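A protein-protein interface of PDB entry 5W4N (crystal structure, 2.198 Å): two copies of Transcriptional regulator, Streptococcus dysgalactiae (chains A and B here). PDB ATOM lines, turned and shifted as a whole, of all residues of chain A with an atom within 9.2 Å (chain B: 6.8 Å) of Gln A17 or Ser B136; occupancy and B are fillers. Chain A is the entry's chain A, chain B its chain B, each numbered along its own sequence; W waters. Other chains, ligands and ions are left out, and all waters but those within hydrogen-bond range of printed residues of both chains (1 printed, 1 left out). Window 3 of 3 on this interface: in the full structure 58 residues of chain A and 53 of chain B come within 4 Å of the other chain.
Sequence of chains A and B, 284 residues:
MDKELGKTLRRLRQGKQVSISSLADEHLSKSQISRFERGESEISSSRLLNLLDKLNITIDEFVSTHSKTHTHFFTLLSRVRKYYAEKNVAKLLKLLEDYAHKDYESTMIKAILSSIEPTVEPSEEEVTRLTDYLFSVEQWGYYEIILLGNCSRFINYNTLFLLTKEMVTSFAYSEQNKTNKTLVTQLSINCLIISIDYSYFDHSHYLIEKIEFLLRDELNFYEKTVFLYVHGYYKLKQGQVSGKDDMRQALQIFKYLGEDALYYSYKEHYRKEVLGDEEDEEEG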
ATOM      1  N   LEU A   9      14.630 -19.964   7.697  1.00  0.00           N
ATOM      2  CA  LEU A   9      14.310 -18.726   8.401  1.00  0.00           C
ATOM      3  C   LEU A   9      15.543 -18.120   9.058  1.00  0.00           C
ATOM      4  O   LEU A   9      15.667 -16.890   9.133  1.00  0.00           O
ATOM      5  CB  LEU A   9      13.215 -18.974   9.435  1.00  0.00           C
ATOM      6  CG  LEU A   9      11.842 -18.455   9.009  1.00  0.00           C
ATOM      7  CD1 LEU A   9      11.821 -16.934   9.041  1.00  0.00           C
ATOM      8  CD2 LEU A   9      11.494 -18.967   7.620  1.00  0.00           C
ATOM      9  N   ARG A  10      16.464 -18.956   9.541  1.00  0.00           N
ATOM     10  CA  ARG A  10      17.661 -18.418  10.181  1.00  0.00           C
ATOM     11  C   ARG A  10      18.545 -17.696   9.169  1.00  0.00           C
ATOM     12  O   ARG A  10      18.994 -16.571   9.416  1.00  0.00           O
ATOM     13  CB  ARG A  10      18.447 -19.528  10.882  1.00  0.00           C
ATOM     14  CG  ARG A  10      19.791 -19.043  11.431  1.00  0.00           C
ATOM     15  CD  ARG A  10      20.447 -20.053  12.359  1.00  0.00           C
ATOM     16  NE  ARG A  10      19.879 -20.016  13.704  1.00  0.00           N
ATOM     17  CZ  ARG A  10      20.409 -20.638  14.751  1.00  0.00           C
ATOM     18  NH1 ARG A  10      21.523 -21.342  14.607  1.00  0.00           N
ATOM     19  NH2 ARG A  10      19.828 -20.557  15.940  1.00  0.00           N
ATOM     20  N   ARG A  11      18.802 -18.323   8.017  1.00  0.00           N
ATOM     21  CA  ARG A  11      19.630 -17.667   7.008  1.00  0.00           C
ATOM     22  C   ARG A  11      18.942 -16.434   6.439  1.00  0.00           C
ATOM     23  O   ARG A  11      19.616 -15.465   6.074  1.00  0.00           O
ATOM     24  CB  ARG A  11      19.998 -18.653   5.895  1.00  0.00           C
ATOM     25  CG  ARG A  11      18.877 -19.017   4.934  1.00  0.00           C
ATOM     26  CD  ARG A  11      19.432 -19.732   3.706  1.00  0.00           C
ATOM     27  NE  ARG A  11      18.410 -19.990   2.693  1.00  0.00           N
ATOM     28  CZ  ARG A  11      17.755 -21.141   2.570  1.00  0.00           C
ATOM     29  NH1 ARG A  11      16.844 -21.289   1.617  1.00  0.00           N
ATOM     30  NH2 ARG A  11      18.010 -22.142   3.401  1.00  0.00           N
ATOM     31  N   LEU A  12      17.609 -16.441   6.372  1.00  0.00           N
ATOM     32  CA  LEU A  12      16.890 -15.244   5.954  1.00  0.00           C
ATOM     33  C   LEU A  12      17.022 -14.137   6.993  1.00  0.00           C
ATOM     34  O   LEU A  12      17.255 -12.975   6.645  1.00  0.00           O
ATOM     35  CB  LEU A  12      15.421 -15.577   5.702  1.00  0.00           C
ATOM     36  CG  LEU A  12      15.086 -16.291   4.389  1.00  0.00           C
ATOM     37  CD1 LEU A  12      13.618 -16.695   4.359  1.00  0.00           C
ATOM     38  CD2 LEU A  12      15.436 -15.416   3.195  1.00  0.00           C
ATOM     39  N   ARG A  13      16.882 -14.482   8.275  1.00  0.00           N
ATOM     40  CA  ARG A  13      17.068 -13.493   9.331  1.00  0.00           C
ATOM     41  C   ARG A  13      18.518 -13.027   9.399  1.00  0.00           C
ATOM     42  O   ARG A  13      18.784 -11.838   9.612  1.00  0.00           O
ATOM     43  CB  ARG A  13      16.619 -14.071  10.673  1.00  0.00           C
ATOM     44  CG  ARG A  13      16.760 -13.110  11.841  1.00  0.00           C
ATOM     45  CD  ARG A  13      16.574 -13.815  13.179  1.00  0.00           C
ATOM     46  NE  ARG A  13      17.394 -15.016  13.293  1.00  0.00           N
ATOM     47  CZ  ARG A  13      18.687 -15.009  13.597  1.00  0.00           C
ATOM     48  NH1 ARG A  13      19.311 -13.860  13.817  1.00  0.00           N
ATOM     49  NH2 ARG A  13      19.358 -16.150  13.678  1.00  0.00           N
ATOM     50  N   GLN A  14      19.468 -13.950   9.217  1.00  0.00           N
ATOM     51  CA  GLN A  14      20.880 -13.576   9.212  1.00  0.00           C
ATOM     52  C   GLN A  14      21.190 -12.613   8.075  1.00  0.00           C
ATOM     53  O   GLN A  14      21.900 -11.619   8.268  1.00  0.00           O
ATOM     54  CB  GLN A  14      21.757 -14.822   9.093  1.00  0.00           C
ATOM     55  CG  GLN A  14      21.844 -15.667  10.347  1.00  0.00           C
ATOM     56  CD  GLN A  14      22.496 -17.008  10.086  1.00  0.00           C
ATOM     57  OE1 GLN A  14      22.641 -17.424   8.935  1.00  0.00           O
ATOM     58  NE2 GLN A  14      22.894 -17.692  11.152  1.00  0.00           N
ATOM     59  N   GLY A  15      20.672 -12.897   6.879  1.00  0.00           N
ATOM     60  CA  GLY A  15      20.929 -12.030   5.742  1.00  0.00           C
ATOM     61  C   GLY A  15      20.379 -10.631   5.923  1.00  0.00           C
ATOM     62  O   GLY A  15      20.934  -9.668   5.391  1.00  0.00           O
ATOM     63  N   LYS A  16      19.287 -10.499   6.671  1.00  0.00           N
ATOM     64  CA  LYS A  16      18.707  -9.198   6.972  1.00  0.00           C
ATOM     65  C   LYS A  16      19.327  -8.551   8.204  1.00  0.00           C
ATOM     66  O   LYS A  16      18.928  -7.439   8.567  1.00  0.00           O
ATOM     67  CB  LYS A  16      17.192  -9.332   7.155  1.00  0.00           C
ATOM     68  CG  LYS A  16      16.432  -9.542   5.852  1.00  0.00           C
ATOM     69  CD  LYS A  16      16.229  -8.228   5.121  1.00  0.00           C
ATOM     70  CE  LYS A  16      15.285  -8.377   3.935  1.00  0.00           C
ATOM     71  NZ  LYS A  16      15.942  -8.988   2.745  1.00  0.00           N
ATOM     72  N   GLN A  17      20.293  -9.218   8.846  1.00  0.00           N
ATOM     73  CA  GLN A  17      21.020  -8.673   9.996  1.00  0.00           C
ATOM     74  C   GLN A  17      20.071  -8.279  11.126  1.00  0.00           C
ATOM     75  O   GLN A  17      20.203  -7.213  11.733  1.00  0.00           O
ATOM     76  CB  GLN A  17      21.899  -7.489   9.582  1.00  0.00           C
ATOM     77  CG  GLN A  17      22.557  -7.652   8.219  1.00  0.00           C
ATOM     78  CD  GLN A  17      23.653  -6.637   7.974  1.00  0.00           C
ATOM     79  OE1 GLN A  17      23.675  -5.964   6.943  1.00  0.00           O
ATOM     80  NE2 GLN A  17      24.575  -6.524   8.922  1.00  0.00           N
ATOM     81  N   VAL A  18      19.112  -9.152  11.420  1.00  0.00           N
ATOM     82  CA  VAL A  18      18.096  -8.911  12.438  1.00  0.00           C
ATOM     83  C   VAL A  18      18.336  -9.859  13.604  1.00  0.00           C
ATOM     84  O   VAL A  18      18.653 -11.037  13.404  1.00  0.00           O
ATOM     85  CB  VAL A  18      16.680  -9.089  11.854  1.00  0.00           C
ATOM     86  CG1 VAL A  18      15.625  -8.858  12.920  1.00  0.00           C
ATOM     87  CG2 VAL A  18      16.468  -8.146  10.682  1.00  0.00           C
ATOM     88  N   SER A  19      18.197  -9.342  14.821  1.00  0.00           N
ATOM     89  CA  SER A  19      18.310 -10.153  16.023  1.00  0.00           C
ATOM     90  C   SER A  19      16.960 -10.774  16.374  1.00  0.00           C
ATOM     91  O   SER A  19      15.905 -10.319  15.929  1.00  0.00           O
ATOM     92  CB  SER A  19      18.826  -9.316  17.194  1.00  0.00           C
ATOM     93  OG  SER A  19      17.929  -8.264  17.502  1.00  0.00           O
ATOM     94  N   ILE A  20      17.007 -11.826  17.193  1.00  0.00           N
ATOM     95  CA  ILE A  20      15.786 -12.568  17.490  1.00  0.00           C
ATOM     96  C   ILE A  20      14.904 -11.822  18.486  1.00  0.00           C
ATOM     97  O   ILE A  20      13.677 -11.974  18.461  1.00  0.00           O
ATOM     98  CB  ILE A  20      16.121 -13.983  17.991  1.00  0.00           C
ATOM     99  CG1 ILE A  20      17.062 -13.919  19.195  1.00  0.00           C
ATOM    100  CG2 ILE A  20      16.733 -14.818  16.874  1.00  0.00           C
ATOM    101  CD1 ILE A  20      17.260 -15.255  19.867  1.00  0.00           C
ATOM    102  N   SER A  22      14.337  -8.642  18.540  1.00  0.00           N
ATOM    103  CA  SER A  22      13.550  -7.666  17.797  1.00  0.00           C
ATOM    104  C   SER A  22      12.402  -8.316  17.035  1.00  0.00           C
ATOM    105  O   SER A  22      11.407  -7.643  16.747  1.00  0.00           O
ATOM    106  CB  SER A  22      14.451  -6.888  16.836  1.00  0.00           C
ATOM    107  OG  SER A  22      14.702  -7.637  15.663  1.00  0.00           O
ATOM    108  N   LEU A  23      12.518  -9.604  16.704  1.00  0.00           N
ATOM    109  CA  LEU A  23      11.409 -10.332  16.099  1.00  0.00           C
ATOM    110  C   LEU A  23      10.415 -10.841  17.132  1.00  0.00           C
ATOM    111  O   LEU A  23       9.247 -11.061  16.794  1.00  0.00           O
ATOM    112  CB  LEU A  23      11.933 -11.514  15.281  1.00  0.00           C
ATOM    113  CG  LEU A  23      12.751 -11.196  14.030  1.00  0.00           C
ATOM    114  CD1 LEU A  23      13.256 -12.482  13.395  1.00  0.00           C
ATOM    115  CD2 LEU A  23      11.928 -10.392  13.037  1.00  0.00           C
ATOM    116  N   LEU A  55      10.685  -9.433   8.839  1.00  0.00           N
ATOM    117  CA  LEU A  55      11.983  -9.437   8.179  1.00  0.00           C
ATOM    118  C   LEU A  55      11.970  -8.705   6.845  1.00  0.00           C
ATOM    119  O   LEU A  55      13.029  -8.582   6.223  1.00  0.00           O
ATOM    120  CB  LEU A  55      12.456 -10.877   7.971  1.00  0.00           C
ATOM    121  CG  LEU A  55      12.888 -11.656   9.214  1.00  0.00           C
ATOM    122  CD1 LEU A  55      13.150 -13.110   8.864  1.00  0.00           C
ATOM    123  CD2 LEU A  55      14.122 -11.021   9.840  1.00  0.00           C
ATOM    124  N   ILE A  57      10.678  -9.760   4.073  1.00  0.00           N
ATOM    125  CA  ILE A  57      10.902 -10.767   3.044  1.00  0.00           C
ATOM    126  C   ILE A  57       9.551 -11.098   2.425  1.00  0.00           C
ATOM    127  O   ILE A  57       8.631 -11.532   3.129  1.00  0.00           O
ATOM    128  CB  ILE A  57      11.568 -12.023   3.624  1.00  0.00           C
ATOM    129  CG1 ILE A  57      13.018 -11.720   4.001  1.00  0.00           C
ATOM    130  CG2 ILE A  57      11.482 -13.182   2.641  1.00  0.00           C
ATOM    131  CD1 ILE A  57      13.594 -12.692   4.985  1.00  0.00           C
ATOM    132  N   TYR B 104      15.355   3.240   7.683  1.00  0.00           N
ATOM    133  CA  TYR B 104      15.509   3.037   6.245  1.00  0.00           C
ATOM    134  C   TYR B 104      14.239   3.416   5.493  1.00  0.00           C
ATOM    135  O   TYR B 104      14.304   4.045   4.429  1.00  0.00           O
ATOM    136  CB  TYR B 104      15.886   1.585   5.953  1.00  0.00           C
ATOM    137  CG  TYR B 104      17.093   1.086   6.717  1.00  0.00           C
ATOM    138  CD1 TYR B 104      18.136   1.943   7.048  1.00  0.00           C
ATOM    139  CD2 TYR B 104      17.192  -0.244   7.099  1.00  0.00           C
ATOM    140  CE1 TYR B 104      19.240   1.488   7.747  1.00  0.00           C
ATOM    141  CE2 TYR B 104      18.291  -0.708   7.794  1.00  0.00           C
ATOM    142  CZ  TYR B 104      19.312   0.162   8.116  1.00  0.00           C
ATOM    143  OH  TYR B 104      20.408  -0.297   8.809  1.00  0.00           O
ATOM    144  N   LEU B 130      21.888   4.247   5.475  1.00  0.00           N
ATOM    145  CA  LEU B 130      21.297   3.290   4.545  1.00  0.00           C
ATOM    146  C   LEU B 130      22.370   2.589   3.721  1.00  0.00           C
ATOM    147  O   LEU B 130      22.357   1.360   3.585  1.00  0.00           O
ATOM    148  CB  LEU B 130      20.293   3.994   3.631  1.00  0.00           C
ATOM    149  CG  LEU B 130      19.768   3.139   2.473  1.00  0.00           C
ATOM    150  CD1 LEU B 130      18.996   1.936   2.995  1.00  0.00           C
ATOM    151  CD2 LEU B 130      18.905   3.963   1.538  1.00  0.00           C
ATOM    152  N   THR B 131      23.309   3.357   3.160  1.00  0.00           N
ATOM    153  CA  THR B 131      24.360   2.754   2.345  1.00  0.00           C
ATOM    154  C   THR B 131      25.250   1.844   3.181  1.00  0.00           C
ATOM    155  O   THR B 131      25.697   0.793   2.704  1.00  0.00           O
ATOM    156  CB  THR B 131      25.192   3.838   1.660  1.00  0.00           C
ATOM    157  OG1 THR B 131      25.733   4.726   2.647  1.00  0.00           O
ATOM    158  CG2 THR B 131      24.334   4.628   0.679  1.00  0.00           C
ATOM    159  N   ASP B 132      25.523   2.231   4.432  1.00  0.00           N
ATOM    160  CA  ASP B 132      26.261   1.349   5.331  1.00  0.00           C
ATOM    161  C   ASP B 132      25.527   0.030   5.525  1.00  0.00           C
ATOM    162  O   ASP B 132      26.151  -1.038   5.560  1.00  0.00           O
ATOM    163  CB  ASP B 132      26.490   2.033   6.679  1.00  0.00           C
ATOM    164  CG  ASP B 132      27.510   3.149   6.603  1.00  0.00           C
ATOM    165  OD1 ASP B 132      28.359   3.117   5.687  1.00  0.00           O
ATOM    166  OD2 ASP B 132      27.468   4.056   7.462  1.00  0.00           O
ATOM    167  N   TYR B 133      24.200   0.083   5.653  1.00  0.00           N
ATOM    168  CA  TYR B 133      23.417  -1.143   5.751  1.00  0.00           C
ATOM    169  C   TYR B 133      23.541  -1.974   4.481  1.00  0.00           C
ATOM    170  O   TYR B 133      23.759  -3.190   4.537  1.00  0.00           O
ATOM    171  CB  TYR B 133      21.951  -0.813   6.031  1.00  0.00           C
ATOM    172  CG  TYR B 133      21.030  -1.992   5.822  1.00  0.00           C
ATOM    173  CD1 TYR B 133      21.022  -3.054   6.715  1.00  0.00           C
ATOM    174  CD2 TYR B 133      20.184  -2.054   4.722  1.00  0.00           C
ATOM    175  CE1 TYR B 133      20.189  -4.141   6.527  1.00  0.00           C
ATOM    176  CE2 TYR B 133      19.346  -3.139   4.523  1.00  0.00           C
ATOM    177  CZ  TYR B 133      19.354  -4.180   5.431  1.00  0.00           C
ATOM    178  OH  TYR B 133      18.525  -5.264   5.245  1.00  0.00           O
ATOM    179  N   LEU B 134      23.405  -1.329   3.319  1.00  0.00           N
ATOM    180  CA  LEU B 134      23.450  -2.058   2.056  1.00  0.00           C
ATOM    181  C   LEU B 134      24.828  -2.660   1.797  1.00  0.00           C
ATOM    182  O   LEU B 134      24.930  -3.710   1.152  1.00  0.00           O
ATOM    183  CB  LEU B 134      23.042  -1.138   0.905  1.00  0.00           C
ATOM    184  CG  LEU B 134      21.603  -0.616   0.940  1.00  0.00           C
ATOM    185  CD1 LEU B 134      21.362   0.376  -0.187  1.00  0.00           C
ATOM    186  CD2 LEU B 134      20.606  -1.765   0.865  1.00  0.00           C
ATOM    187  N   PHE B 135      25.892  -2.019   2.289  1.00  0.00           N
ATOM    188  CA  PHE B 135      27.227  -2.595   2.149  1.00  0.00           C
ATOM    189  C   PHE B 135      27.408  -3.816   3.041  1.00  0.00           C
ATOM    190  O   PHE B 135      28.123  -4.754   2.671  1.00  0.00           O
ATOM    191  CB  PHE B 135      28.296  -1.552   2.478  1.00  0.00           C
ATOM    192  CG  PHE B 135      28.698  -0.700   1.309  1.00  0.00           C
ATOM    193  CD1 PHE B 135      29.180  -1.277   0.145  1.00  0.00           C
ATOM    194  CD2 PHE B 135      28.608   0.681   1.378  1.00  0.00           C
ATOM    195  CE1 PHE B 135      29.555  -0.492  -0.931  1.00  0.00           C
ATOM    196  CE2 PHE B 135      28.981   1.469   0.307  1.00  0.00           C
ATOM    197  CZ  PHE B 135      29.455   0.883  -0.849  1.00  0.00           C
ATOM    198  N   SER B 136      26.779  -3.820   4.216  1.00  0.00           N
ATOM    199  CA  SER B 136      26.881  -4.943   5.138  1.00  0.00           C
ATOM    200  C   SER B 136      25.984  -6.112   4.751  1.00  0.00           C
ATOM    201  O   SER B 136      26.143  -7.203   5.306  1.00  0.00           O
ATOM    202  CB  SER B 136      26.547  -4.484   6.560  1.00  0.00           C
ATOM    203  OG  SER B 136      25.235  -3.956   6.628  1.00  0.00           O
ATOM    204  N   VAL B 137      25.056  -5.915   3.820  1.00  0.00           N
ATOM    205  CA  VAL B 137      24.190  -6.992   3.354  1.00  0.00           C
ATOM    206  C   VAL B 137      24.950  -7.828   2.335  1.00  0.00           C
ATOM    207  O   VAL B 137      25.637  -7.288   1.458  1.00  0.00           O
ATOM    208  CB  VAL B 137      22.893  -6.422   2.753  1.00  0.00           C
ATOM    209  CG1 VAL B 137      22.311  -7.369   1.721  1.00  0.00           C
ATOM    210  CG2 VAL B 137      21.876  -6.135   3.846  1.00  0.00           C
ATOM    211  N   GLU B 138      24.839  -9.155   2.453  1.00  0.00           N
ATOM    212  CA  GLU B 138      25.463 -10.055   1.494  1.00  0.00           C
ATOM    213  C   GLU B 138      24.469 -10.825   0.636  1.00  0.00           C
ATOM    214  O   GLU B 138      24.861 -11.348  -0.411  1.00  0.00           O
ATOM    215  CB  GLU B 138      26.386 -11.052   2.208  1.00  0.00           C
ATOM    216  CG  GLU B 138      27.380 -10.377   3.136  1.00  0.00           C
ATOM    217  CD  GLU B 138      27.884 -11.299   4.224  1.00  0.00           C
ATOM    218  OE1 GLU B 138      27.362 -12.427   4.339  1.00  0.00           O
ATOM    219  OE2 GLU B 138      28.782 -10.884   4.983  1.00  0.00           O
ATOM    220  N   GLN B 139      23.205 -10.902   1.038  1.00  0.00           N
ATOM    221  CA  GLN B 139      22.133 -11.417   0.185  1.00  0.00           C
ATOM    222  C   GLN B 139      21.150 -10.277  -0.066  1.00  0.00           C
ATOM    223  O   GLN B 139      20.301  -9.972   0.778  1.00  0.00           O
ATOM    224  CB  GLN B 139      21.452 -12.640   0.797  1.00  0.00           C
ATOM    225  CG  GLN B 139      21.411 -12.695   2.309  1.00  0.00           C
ATOM    226  CD  GLN B 139      21.078 -14.093   2.816  1.00  0.00           C
ATOM    227  OE1 GLN B 139      20.127 -14.729   2.352  1.00  0.00           O
ATOM    228  NE2 GLN B 139      21.865 -14.578   3.769  1.00  0.00           N
ATOM    229  N   LEU B 163      27.663  -0.119  -4.733  1.00  0.00           N
ATOM    230  CA  LEU B 163      26.485  -0.852  -4.279  1.00  0.00           C
ATOM    231  C   LEU B 163      25.864  -1.652  -5.416  1.00  0.00           C
ATOM    232  O   LEU B 163      25.440  -2.797  -5.220  1.00  0.00           O
ATOM    233  CB  LEU B 163      25.459   0.115  -3.688  1.00  0.00           C
ATOM    234  CG  LEU B 163      25.815   0.775  -2.355  1.00  0.00           C
ATOM    235  CD1 LEU B 163      24.785   1.839  -1.993  1.00  0.00           C
ATOM    236  CD2 LEU B 163      25.928  -0.270  -1.256  1.00  0.00           C
ATOM    237  N   GLU B 166      27.837  -4.836  -6.085  1.00  0.00           N
ATOM    238  CA  GLU B 166      27.614  -5.842  -5.053  1.00  0.00           C
ATOM    239  C   GLU B 166      26.213  -6.431  -5.153  1.00  0.00           C
ATOM    240  O   GLU B 166      26.022  -7.631  -4.927  1.00  0.00           O
ATOM    241  CB  GLU B 166      27.852  -5.235  -3.670  1.00  0.00           C
ATOM    242  CG  GLU B 166      29.311  -4.906  -3.391  1.00  0.00           C
ATOM    243  CD  GLU B 166      29.560  -4.523  -1.947  1.00  0.00           C
ATOM    244  OE1 GLU B 166      28.629  -4.645  -1.123  1.00  0.00           O
ATOM    245  OE2 GLU B 166      30.691  -4.095  -1.634  1.00  0.00           O
HETATM  246  O   HOH W   1      23.454 -10.116   4.179  1.00  0.00           O
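Printed residues of chain B within 4 Å of Gly A15: Val B137 (3.97 Å) and Gln B139 (3.4 Å). Of the printed residues of chain B, Lys A16 touches Tyr B133. Of chain B, only Tyr B133 (3.7 Å), Ser B136 (2.6 Å) and Val B137 (3.4 Å) come within 4 Å of Gln A17. Ser B136 touches just one residue of chain A: Gln A17. Val B137 touches just these residues of chain A: Gly A15 (3.97 Å) and Gln A17 (3.4 Å). Printed residues of chain A within 4 Å of Gln B139: Arg A11 (3.3 Å) and Gly A15 (3.4 Å). Leu B163 touches none of the printed residues of chain A. The nearest residue of chain A that does not touch Ser B136 is Gly A15 (5.8 Å).
Of the 16 printed residues of chain A, 4 touch a printed residue of chain B. Printed residues of chain B that touch a printed residue of chain A: Tyr B133, Ser B136, Val B137 and Gln B139. Hydrophobic or aromatic side chains of chain B within 4 Å of the printed part of chain A: Tyr B133 and Val B137.
No position is printed for both chains.
The backbone carbonyl oxygen (O) of Arg A11 is in hydrogen-bond range of the side-chain amide nitrogen (NE2) of Gln B139, at 3.3 Å. The side-chain amide oxygen (OE1) of Gln A17 sits at hydrogen-bond distance from the side-chain hydroxyl (OG) of Ser B136 (2.6 Å). N of Val B137 sits at hydrogen-bond distance from OE1 of Gln A17.
Among the printed residues, merely in contact across the chains: Gly A15 with Gln B139 (3.4 Å), Gln A17 with Tyr B133 (3.7 Å), Lys A16 with Tyr B133 (3.8 Å) and Gly A15 with Val B137 (3.97 Å).
O of Tyr B133 sits at hydrogen-bond distance from OG of Ser B136 (2.7 Å). OG of Ser B136 lies within hydrogen-bond range of O of Asp B132 (3.2 Å).
Water W1 lies within hydrogen-bond range of the backbone NH (N) of Glu B138, the backbone carbonyl oxygen (O) of Gly A15 and the backbone NH (N) of Gln B139.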
